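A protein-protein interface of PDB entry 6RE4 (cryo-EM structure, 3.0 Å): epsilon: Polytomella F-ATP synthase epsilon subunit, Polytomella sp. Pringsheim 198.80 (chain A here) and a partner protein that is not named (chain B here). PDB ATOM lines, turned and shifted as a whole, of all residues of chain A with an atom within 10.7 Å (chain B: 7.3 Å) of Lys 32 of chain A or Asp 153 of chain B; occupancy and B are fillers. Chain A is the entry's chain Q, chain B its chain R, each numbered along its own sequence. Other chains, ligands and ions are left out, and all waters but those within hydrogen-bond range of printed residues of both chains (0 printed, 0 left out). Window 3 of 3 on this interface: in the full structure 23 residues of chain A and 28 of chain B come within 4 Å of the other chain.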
ATOM      1  N   LEU A  26     -32.236   1.180  -5.753  1.00  0.00           N
ATOM      2  CA  LEU A  26     -32.277   1.284  -7.204  1.00  0.00           C
ATOM      3  C   LEU A  26     -31.377   0.280  -7.896  1.00  0.00           C
ATOM      4  O   LEU A  26     -31.717  -0.174  -8.988  1.00  0.00           O
ATOM      5  CB  LEU A  26     -31.890   2.694  -7.627  1.00  0.00           C
ATOM      6  CG  LEU A  26     -32.961   3.746  -7.879  1.00  0.00           C
ATOM      7  CD1 LEU A  26     -33.871   3.982  -6.704  1.00  0.00           C
ATOM      8  CD2 LEU A  26     -32.205   4.994  -8.134  1.00  0.00           C
ATOM      9  N   LEU A  27     -30.246  -0.075  -7.302  1.00  0.00           N
ATOM     10  CA  LEU A  27     -29.434  -1.118  -7.905  1.00  0.00           C
ATOM     11  C   LEU A  27     -30.053  -2.490  -7.703  1.00  0.00           C
ATOM     12  O   LEU A  27     -29.893  -3.369  -8.554  1.00  0.00           O
ATOM     13  CB  LEU A  27     -28.019  -1.083  -7.334  1.00  0.00           C
ATOM     14  CG  LEU A  27     -26.972  -2.037  -7.900  1.00  0.00           C
ATOM     15  CD1 LEU A  27     -26.993  -2.013  -9.402  1.00  0.00           C
ATOM     16  CD2 LEU A  27     -25.614  -1.637  -7.402  1.00  0.00           C
ATOM     17  N   ARG A  28     -30.770  -2.691  -6.600  1.00  0.00           N
ATOM     18  CA  ARG A  28     -31.444  -3.970  -6.407  1.00  0.00           C
ATOM     19  C   ARG A  28     -32.629  -4.128  -7.344  1.00  0.00           C
ATOM     20  O   ARG A  28     -32.921  -5.247  -7.777  1.00  0.00           O
ATOM     21  CB  ARG A  28     -31.895  -4.119  -4.958  1.00  0.00           C
ATOM     22  CG  ARG A  28     -30.763  -4.424  -4.012  1.00  0.00           C
ATOM     23  CD  ARG A  28     -31.258  -4.635  -2.615  1.00  0.00           C
ATOM     24  NE  ARG A  28     -30.245  -4.241  -1.652  1.00  0.00           N
ATOM     25  CZ  ARG A  28     -30.361  -3.198  -0.845  1.00  0.00           C
ATOM     26  NH1 ARG A  28     -31.448  -2.443  -0.888  1.00  0.00           N
ATOM     27  NH2 ARG A  28     -29.394  -2.905   0.005  1.00  0.00           N
ATOM     28  N   ASN A  29     -33.298  -3.030  -7.694  1.00  0.00           N
ATOM     29  CA  ASN A  29     -34.472  -3.107  -8.556  1.00  0.00           C
ATOM     30  C   ASN A  29     -34.150  -3.456 -10.007  1.00  0.00           C
ATOM     31  O   ASN A  29     -35.073  -3.774 -10.764  1.00  0.00           O
ATOM     32  CB  ASN A  29     -35.237  -1.784  -8.513  1.00  0.00           C
ATOM     33  CG  ASN A  29     -35.916  -1.553  -7.181  1.00  0.00           C
ATOM     34  OD1 ASN A  29     -36.050  -2.473  -6.379  1.00  0.00           O
ATOM     35  ND2 ASN A  29     -36.346  -0.321  -6.937  1.00  0.00           N
ATOM     36  N   VAL A  30     -32.887  -3.423 -10.420  1.00  0.00           N
ATOM     37  CA  VAL A  30     -32.544  -3.668 -11.816  1.00  0.00           C
ATOM     38  C   VAL A  30     -31.659  -4.899 -11.937  1.00  0.00           C
ATOM     39  O   VAL A  30     -30.770  -4.966 -12.791  1.00  0.00           O
ATOM     40  CB  VAL A  30     -31.886  -2.428 -12.451  1.00  0.00           C
ATOM     41  CG1 VAL A  30     -32.902  -1.310 -12.547  1.00  0.00           C
ATOM     42  CG2 VAL A  30     -30.694  -1.957 -11.634  1.00  0.00           C
ATOM     43  N   LEU A  31     -31.911  -5.891 -11.096  1.00  0.00           N
ATOM     44  CA  LEU A  31     -31.181  -7.146 -11.119  1.00  0.00           C
ATOM     45  C   LEU A  31     -31.988  -8.234 -11.817  1.00  0.00           C
ATOM     46  O   LEU A  31     -33.156  -8.057 -12.167  1.00  0.00           O
ATOM     47  CB  LEU A  31     -30.841  -7.581  -9.696  1.00  0.00           C
ATOM     48  CG  LEU A  31     -29.803  -6.710  -9.009  1.00  0.00           C
ATOM     49  CD1 LEU A  31     -29.657  -7.114  -7.563  1.00  0.00           C
ATOM     50  CD2 LEU A  31     -28.495  -6.856  -9.747  1.00  0.00           C
ATOM     51  N   LYS A  32     -31.342  -9.378 -12.014  1.00  0.00           N
ATOM     52  CA  LYS A  32     -32.020 -10.546 -12.550  1.00  0.00           C
ATOM     53  C   LYS A  32     -32.848 -11.229 -11.467  1.00  0.00           C
ATOM     54  O   LYS A  32     -32.470 -11.269 -10.297  1.00  0.00           O
ATOM     55  CB  LYS A  32     -31.013 -11.533 -13.135  1.00  0.00           C
ATOM     56  CG  LYS A  32     -30.380 -11.063 -14.424  1.00  0.00           C
ATOM     57  CD  LYS A  32     -29.802 -12.227 -15.209  1.00  0.00           C
ATOM     58  CE  LYS A  32     -28.417 -12.604 -14.718  1.00  0.00           C
ATOM     59  NZ  LYS A  32     -27.356 -11.820 -15.406  1.00  0.00           N
ATOM     60  N   GLU A  33     -33.994 -11.761 -11.874  1.00  0.00           N
ATOM     61  CA  GLU A  33     -34.957 -12.421 -10.991  1.00  0.00           C
ATOM     62  C   GLU A  33     -34.482 -13.686 -10.264  1.00  0.00           C
ATOM     63  O   GLU A  33     -35.099 -14.043  -9.251  1.00  0.00           O
ATOM     64  CB  GLU A  33     -36.231 -12.736 -11.776  1.00  0.00           C
ATOM     65  CG  GLU A  33     -37.051 -11.499 -12.106  1.00  0.00           C
ATOM     66  CD  GLU A  33     -37.590 -10.809 -10.869  1.00  0.00           C
ATOM     67  OE1 GLU A  33     -37.976 -11.512  -9.913  1.00  0.00           O
ATOM     68  OE2 GLU A  33     -37.627  -9.563 -10.847  1.00  0.00           O
ATOM     69  N   PRO A  34     -33.455 -14.420 -10.726  1.00  0.00           N
ATOM     70  CA  PRO A  34     -32.783 -15.341  -9.790  1.00  0.00           C
ATOM     71  C   PRO A  34     -32.134 -14.650  -8.603  1.00  0.00           C
ATOM     72  O   PRO A  34     -32.020 -15.254  -7.530  1.00  0.00           O
ATOM     73  CB  PRO A  34     -31.747 -16.032 -10.678  1.00  0.00           C
ATOM     74  CG  PRO A  34     -32.413 -16.126 -11.965  1.00  0.00           C
ATOM     75  CD  PRO A  34     -33.224 -14.862 -12.117  1.00  0.00           C
ATOM     76  N   PHE A  35     -31.693 -13.400  -8.766  1.00  0.00           N
ATOM     77  CA  PHE A  35     -31.061 -12.666  -7.683  1.00  0.00           C
ATOM     78  C   PHE A  35     -31.873 -11.487  -7.172  1.00  0.00           C
ATOM     79  O   PHE A  35     -31.614 -11.027  -6.056  1.00  0.00           O
ATOM     80  CB  PHE A  35     -29.684 -12.168  -8.126  1.00  0.00           C
ATOM     81  CG  PHE A  35     -28.760 -13.265  -8.538  1.00  0.00           C
ATOM     82  CD1 PHE A  35     -28.109 -14.027  -7.587  1.00  0.00           C
ATOM     83  CD2 PHE A  35     -28.547 -13.540  -9.873  1.00  0.00           C
ATOM     84  CE1 PHE A  35     -27.257 -15.045  -7.959  1.00  0.00           C
ATOM     85  CE2 PHE A  35     -27.689 -14.548 -10.253  1.00  0.00           C
ATOM     86  CZ  PHE A  35     -27.045 -15.304  -9.295  1.00  0.00           C
ATOM     87  N   LYS A  36     -32.838 -10.985  -7.946  1.00  0.00           N
ATOM     88  CA  LYS A  36     -33.692  -9.914  -7.443  1.00  0.00           C
ATOM     89  C   LYS A  36     -34.613 -10.413  -6.339  1.00  0.00           C
ATOM     90  O   LYS A  36     -34.889  -9.681  -5.383  1.00  0.00           O
ATOM     91  CB  LYS A  36     -34.505  -9.306  -8.586  1.00  0.00           C
ATOM     92  CG  LYS A  36     -35.371  -8.125  -8.194  1.00  0.00           C
ATOM     93  CD  LYS A  36     -35.649  -7.234  -9.390  1.00  0.00           C
ATOM     94  CE  LYS A  36     -36.709  -6.192  -9.076  1.00  0.00           C
ATOM     95  NZ  LYS A  36     -36.582  -5.680  -7.686  1.00  0.00           N
ATOM     96  N   ALA A  37     -35.069 -11.662  -6.437  1.00  0.00           N
ATOM     97  CA  ALA A  37     -35.899 -12.226  -5.382  1.00  0.00           C
ATOM     98  C   ALA A  37     -35.087 -12.518  -4.129  1.00  0.00           C
ATOM     99  O   ALA A  37     -35.642 -12.569  -3.028  1.00  0.00           O
ATOM    100  CB  ALA A  37     -36.594 -13.489  -5.880  1.00  0.00           C
ATOM    101  N   LYS A  38     -33.777 -12.714  -4.276  1.00  0.00           N
ATOM    102  CA  LYS A  38     -32.916 -12.836  -3.108  1.00  0.00           C
ATOM    103  C   LYS A  38     -32.654 -11.480  -2.469  1.00  0.00           C
ATOM    104  O   LYS A  38     -32.786 -11.343  -1.249  1.00  0.00           O
ATOM    105  CB  LYS A  38     -31.602 -13.514  -3.501  1.00  0.00           C
ATOM    106  CG  LYS A  38     -30.729 -13.955  -2.338  1.00  0.00           C
ATOM    107  CD  LYS A  38     -29.596 -12.981  -2.013  1.00  0.00           C
ATOM    108  CE  LYS A  38     -28.747 -13.527  -0.883  1.00  0.00           C
ATOM    109  NZ  LYS A  38     -27.618 -12.647  -0.524  1.00  0.00           N
ATOM    110  N   ALA A  39     -32.330 -10.463  -3.271  1.00  0.00           N
ATOM    111  CA  ALA A  39     -32.084  -9.120  -2.755  1.00  0.00           C
ATOM    112  C   ALA A  39     -33.363  -8.383  -2.380  1.00  0.00           C
ATOM    113  O   ALA A  39     -33.289  -7.259  -1.879  1.00  0.00           O
ATOM    114  CB  ALA A  39     -31.304  -8.303  -3.779  1.00  0.00           C
ATOM    115  N   GLN A  40     -34.524  -8.989  -2.618  1.00  0.00           N
ATOM    116  CA  GLN A  40     -35.793  -8.479  -2.125  1.00  0.00           C
ATOM    117  C   GLN A  40     -35.869  -8.506  -0.603  1.00  0.00           C
ATOM    118  O   GLN A  40     -36.617  -7.718  -0.017  1.00  0.00           O
ATOM    119  CB  GLN A  40     -36.920  -9.323  -2.727  1.00  0.00           C
ATOM    120  CG  GLN A  40     -38.308  -8.731  -2.662  1.00  0.00           C
ATOM    121  CD  GLN A  40     -38.438  -7.467  -3.469  1.00  0.00           C
ATOM    122  OE1 GLN A  40     -38.558  -6.376  -2.919  1.00  0.00           O
ATOM    123  NE2 GLN A  40     -38.421  -7.609  -4.787  1.00  0.00           N
ATOM    124  N   ARG A  42     -33.377  -7.935   1.777  1.00  0.00           N
ATOM    125  CA  ARG A  42     -32.625  -6.883   2.448  1.00  0.00           C
ATOM    126  C   ARG A  42     -33.095  -5.486   2.088  1.00  0.00           C
ATOM    127  O   ARG A  42     -32.349  -4.524   2.282  1.00  0.00           O
ATOM    128  CB  ARG A  42     -31.141  -7.024   2.133  1.00  0.00           C
ATOM    129  CG  ARG A  42     -30.830  -6.900   0.683  1.00  0.00           C
ATOM    130  CD  ARG A  42     -29.364  -6.704   0.485  1.00  0.00           C
ATOM    131  NE  ARG A  42     -28.644  -7.963   0.406  1.00  0.00           N
ATOM    132  CZ  ARG A  42     -28.239  -8.505  -0.734  1.00  0.00           C
ATOM    133  NH1 ARG A  42     -27.583  -9.648  -0.731  1.00  0.00           N
ATOM    134  NH2 ARG A  42     -28.484  -7.901  -1.880  1.00  0.00           N
ATOM    135  N   LYS B 126     -14.514  -8.240 -10.831  1.00  0.00           N
ATOM    136  CA  LYS B 126     -15.170  -6.977 -11.147  1.00  0.00           C
ATOM    137  C   LYS B 126     -16.571  -6.981 -10.558  1.00  0.00           C
ATOM    138  O   LYS B 126     -17.456  -7.683 -11.054  1.00  0.00           O
ATOM    139  CB  LYS B 126     -15.236  -6.732 -12.650  1.00  0.00           C
ATOM    140  CG  LYS B 126     -13.909  -6.507 -13.328  1.00  0.00           C
ATOM    141  CD  LYS B 126     -14.105  -5.793 -14.659  1.00  0.00           C
ATOM    142  CE  LYS B 126     -15.065  -6.549 -15.559  1.00  0.00           C
ATOM    143  NZ  LYS B 126     -15.003  -6.085 -16.965  1.00  0.00           N
ATOM    144  N   ALA B 150     -23.499  -5.296  -6.619  1.00  0.00           N
ATOM    145  CA  ALA B 150     -24.162  -6.195  -7.555  1.00  0.00           C
ATOM    146  C   ALA B 150     -23.220  -6.454  -8.719  1.00  0.00           C
ATOM    147  O   ALA B 150     -23.039  -5.581  -9.569  1.00  0.00           O
ATOM    148  CB  ALA B 150     -25.469  -5.579  -8.037  1.00  0.00           C
ATOM    149  N   THR B 151     -22.643  -7.652  -8.769  1.00  0.00           N
ATOM    150  CA  THR B 151     -21.638  -7.964  -9.774  1.00  0.00           C
ATOM    151  C   THR B 151     -22.251  -8.021 -11.175  1.00  0.00           C
ATOM    152  O   THR B 151     -23.466  -8.087 -11.352  1.00  0.00           O
ATOM    153  CB  THR B 151     -20.931  -9.274  -9.442  1.00  0.00           C
ATOM    154  OG1 THR B 151     -19.920  -9.528 -10.424  1.00  0.00           O
ATOM    155  CG2 THR B 151     -21.911 -10.420  -9.408  1.00  0.00           C
ATOM    156  N   LEU B 152     -21.377  -7.952 -12.181  1.00  0.00           N
ATOM    157  CA  LEU B 152     -21.813  -7.634 -13.538  1.00  0.00           C
ATOM    158  C   LEU B 152     -22.524  -8.781 -14.236  1.00  0.00           C
ATOM    159  O   LEU B 152     -23.313  -8.533 -15.152  1.00  0.00           O
ATOM    160  CB  LEU B 152     -20.617  -7.200 -14.370  1.00  0.00           C
ATOM    161  CG  LEU B 152     -19.924  -5.972 -13.808  1.00  0.00           C
ATOM    162  CD1 LEU B 152     -18.503  -5.955 -14.275  1.00  0.00           C
ATOM    163  CD2 LEU B 152     -20.659  -4.731 -14.268  1.00  0.00           C
ATOM    164  N   ASP B 153     -22.268 -10.019 -13.848  1.00  0.00           N
ATOM    165  CA  ASP B 153     -22.951 -11.142 -14.466  1.00  0.00           C
ATOM    166  C   ASP B 153     -24.264 -11.496 -13.782  1.00  0.00           C
ATOM    167  O   ASP B 153     -24.815 -12.568 -14.051  1.00  0.00           O
ATOM    168  CB  ASP B 153     -22.020 -12.355 -14.531  1.00  0.00           C
ATOM    169  CG  ASP B 153     -21.256 -12.579 -13.249  1.00  0.00           C
ATOM    170  OD1 ASP B 153     -21.771 -12.250 -12.162  1.00  0.00           O
ATOM    171  OD2 ASP B 153     -20.117 -13.079 -13.333  1.00  0.00           O
ATOM    172  N   GLN B 154     -24.771 -10.634 -12.899  1.00  0.00           N
ATOM    173  CA  GLN B 154     -26.116 -10.794 -12.360  1.00  0.00           C
ATOM    174  C   GLN B 154     -26.978  -9.548 -12.534  1.00  0.00           C
ATOM    175  O   GLN B 154     -28.050  -9.458 -11.924  1.00  0.00           O
ATOM    176  CB  GLN B 154     -26.065 -11.200 -10.887  1.00  0.00           C
ATOM    177  CG  GLN B 154     -25.571 -10.145  -9.952  1.00  0.00           C
ATOM    178  CD  GLN B 154     -25.649 -10.583  -8.519  1.00  0.00           C
ATOM    179  OE1 GLN B 154     -24.898 -11.453  -8.082  1.00  0.00           O
ATOM    180  NE2 GLN B 154     -26.565  -9.981  -7.770  1.00  0.00           N
ATOM    181  N   VAL B 155     -26.566  -8.605 -13.356  1.00  0.00           N
ATOM    182  CA  VAL B 155     -27.387  -7.440 -13.648  1.00  0.00           C
ATOM    183  C   VAL B 155     -28.162  -7.716 -14.933  1.00  0.00           C
ATOM    184  O   VAL B 155     -27.691  -8.445 -15.816  1.00  0.00           O
ATOM    185  CB  VAL B 155     -26.521  -6.157 -13.729  1.00  0.00           C
ATOM    186  CG1 VAL B 155     -25.589  -6.162 -14.930  1.00  0.00           C
ATOM    187  CG2 VAL B 155     -27.375  -4.905 -13.710  1.00  0.00           C
ATOM    188  N   ASP B 156     -29.502  -7.152 -15.020  1.00  0.00           N
ATOM    189  CA  ASP B 156     -29.980  -7.388 -16.375  1.00  0.00           C
ATOM    190  C   ASP B 156     -29.727  -6.167 -17.255  1.00  0.00           C
ATOM    191  O   ASP B 156     -29.681  -5.038 -16.763  1.00  0.00           O
ATOM    192  CB  ASP B 156     -31.474  -7.771 -16.387  1.00  0.00           C
ATOM    193  CG  ASP B 156     -32.418  -6.691 -15.826  1.00  0.00           C
ATOM    194  OD1 ASP B 156     -31.990  -5.655 -15.293  1.00  0.00           O
ATOM    195  OD2 ASP B 156     -33.643  -6.903 -15.928  1.00  0.00           O
ATOM    196  N   PRO B 157     -29.490  -6.344 -18.552  1.00  0.00           N
ATOM    197  CA  PRO B 157     -29.302  -5.186 -19.427  1.00  0.00           C
ATOM    198  C   PRO B 157     -30.586  -4.638 -20.017  1.00  0.00           C
ATOM    199  O   PRO B 157     -30.514  -3.742 -20.862  1.00  0.00           O
ATOM    200  CB  PRO B 157     -28.404  -5.753 -20.529  1.00  0.00           C
ATOM    201  CG  PRO B 157     -28.859  -7.143 -20.657  1.00  0.00           C
ATOM    202  CD  PRO B 157     -29.230  -7.604 -19.270  1.00  0.00           C
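The side-chain amino group (NZ) of Lys 32 of chain A sits at hydrogen-bond distance from the backbone carbonyl oxygen (O) of Asp 153 of chain B (3.0 Å). N of Lys 32 of chain A sits at hydrogen-bond distance from O of Gln 154 of chain B, 3.3 Å away. The backbone carbonyl oxygen of Val 155 of chain B is in hydrogen-bond range of the side-chain amino group of Lys 32 of chain A, at 3.4 Å. The backbone carbonyl oxygen (O) of Val 30 of chain A is in hydrogen-bond range of the backbone NH (N) of Asp 156 of chain B (3.4 Å).
Hydrophobic or aromatic side chains of chain A that line the printed part of chain B: Leu 27, Leu 31 and Phe 35. Of the 9 printed residues of chain B, 5 touch a printed residue of chain A. Hydrophobic or aromatic side chains of chain B within 4 Å of the printed part of chain A: Ala 150 and Val 155. Among the printed residues, 11 pairs touch across the chains. Among the printed residues, no Asp or Glu carboxylate lies within 4 Å of a Lys or Arg side-chain nitrogen of the other chain.
Printed residues of chain B within 4 Å of Val 30 of chain A: Val 155 (3.5 Å) and Asp 156 (2.9 Å). Of the printed residues of chain B, Lys 32 of chain A touches Asp 153 (3.0 Å), Gln 154 (3.3 Å), Val 155 (3.4 Å) and Asp 156 (3.99 Å). Pro 34 of chain A touches none of the printed residues of chain B. Of the printed residues of chain B, Phe 35 of chain A touches Gln 154 (3.6 Å). No residue of chain A comes within 4 Å of Thr 151 of chain B. No residue of chain A comes within 4 Å of Leu 152 of chain B. Of chain A, only Lys 32 comes within 4 Å of Asp 153 of chain B. Gln 154 of chain B touches just these residues of chain A: Leu 31 (3.4 Å), Lys 32 (3.3 Å) and Phe 35 (3.6 Å). Val 155 of chain B touches just these residues of chain A: Val 30 and Lys 32. Printed residues of chain A within 4 Å of Asp 156 of chain B: Val 30 (2.9 Å), Leu 31 (3.96 Å) and Lys 32 (3.99 Å). Pro 157 of chain B touches none of the printed residues of chain A. The nearest printed residue of chain B that does not touch Lys 32 of chain A is Leu 152 of chain B (5.2 Å). The nearest residue of chain A that does not touch Asp 153 of chain B is Phe 35 of chain A (5.2 Å).
Among the printed residues, merely in contact across the chains: Leu 31 of chain A with Gln 154 of chain B, Val 30 of chain A with Val 155 of chain B, Phe 35 of chain A with Gln 154 of chain B, Leu 31 of chain A with Ala 150 of chain B, Leu 27 of chain A with Ala 150 of chain B, Leu 31 of chain A with Asp 156 of chain B and Lys 32 of chain A with Asp 156 of chain B.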
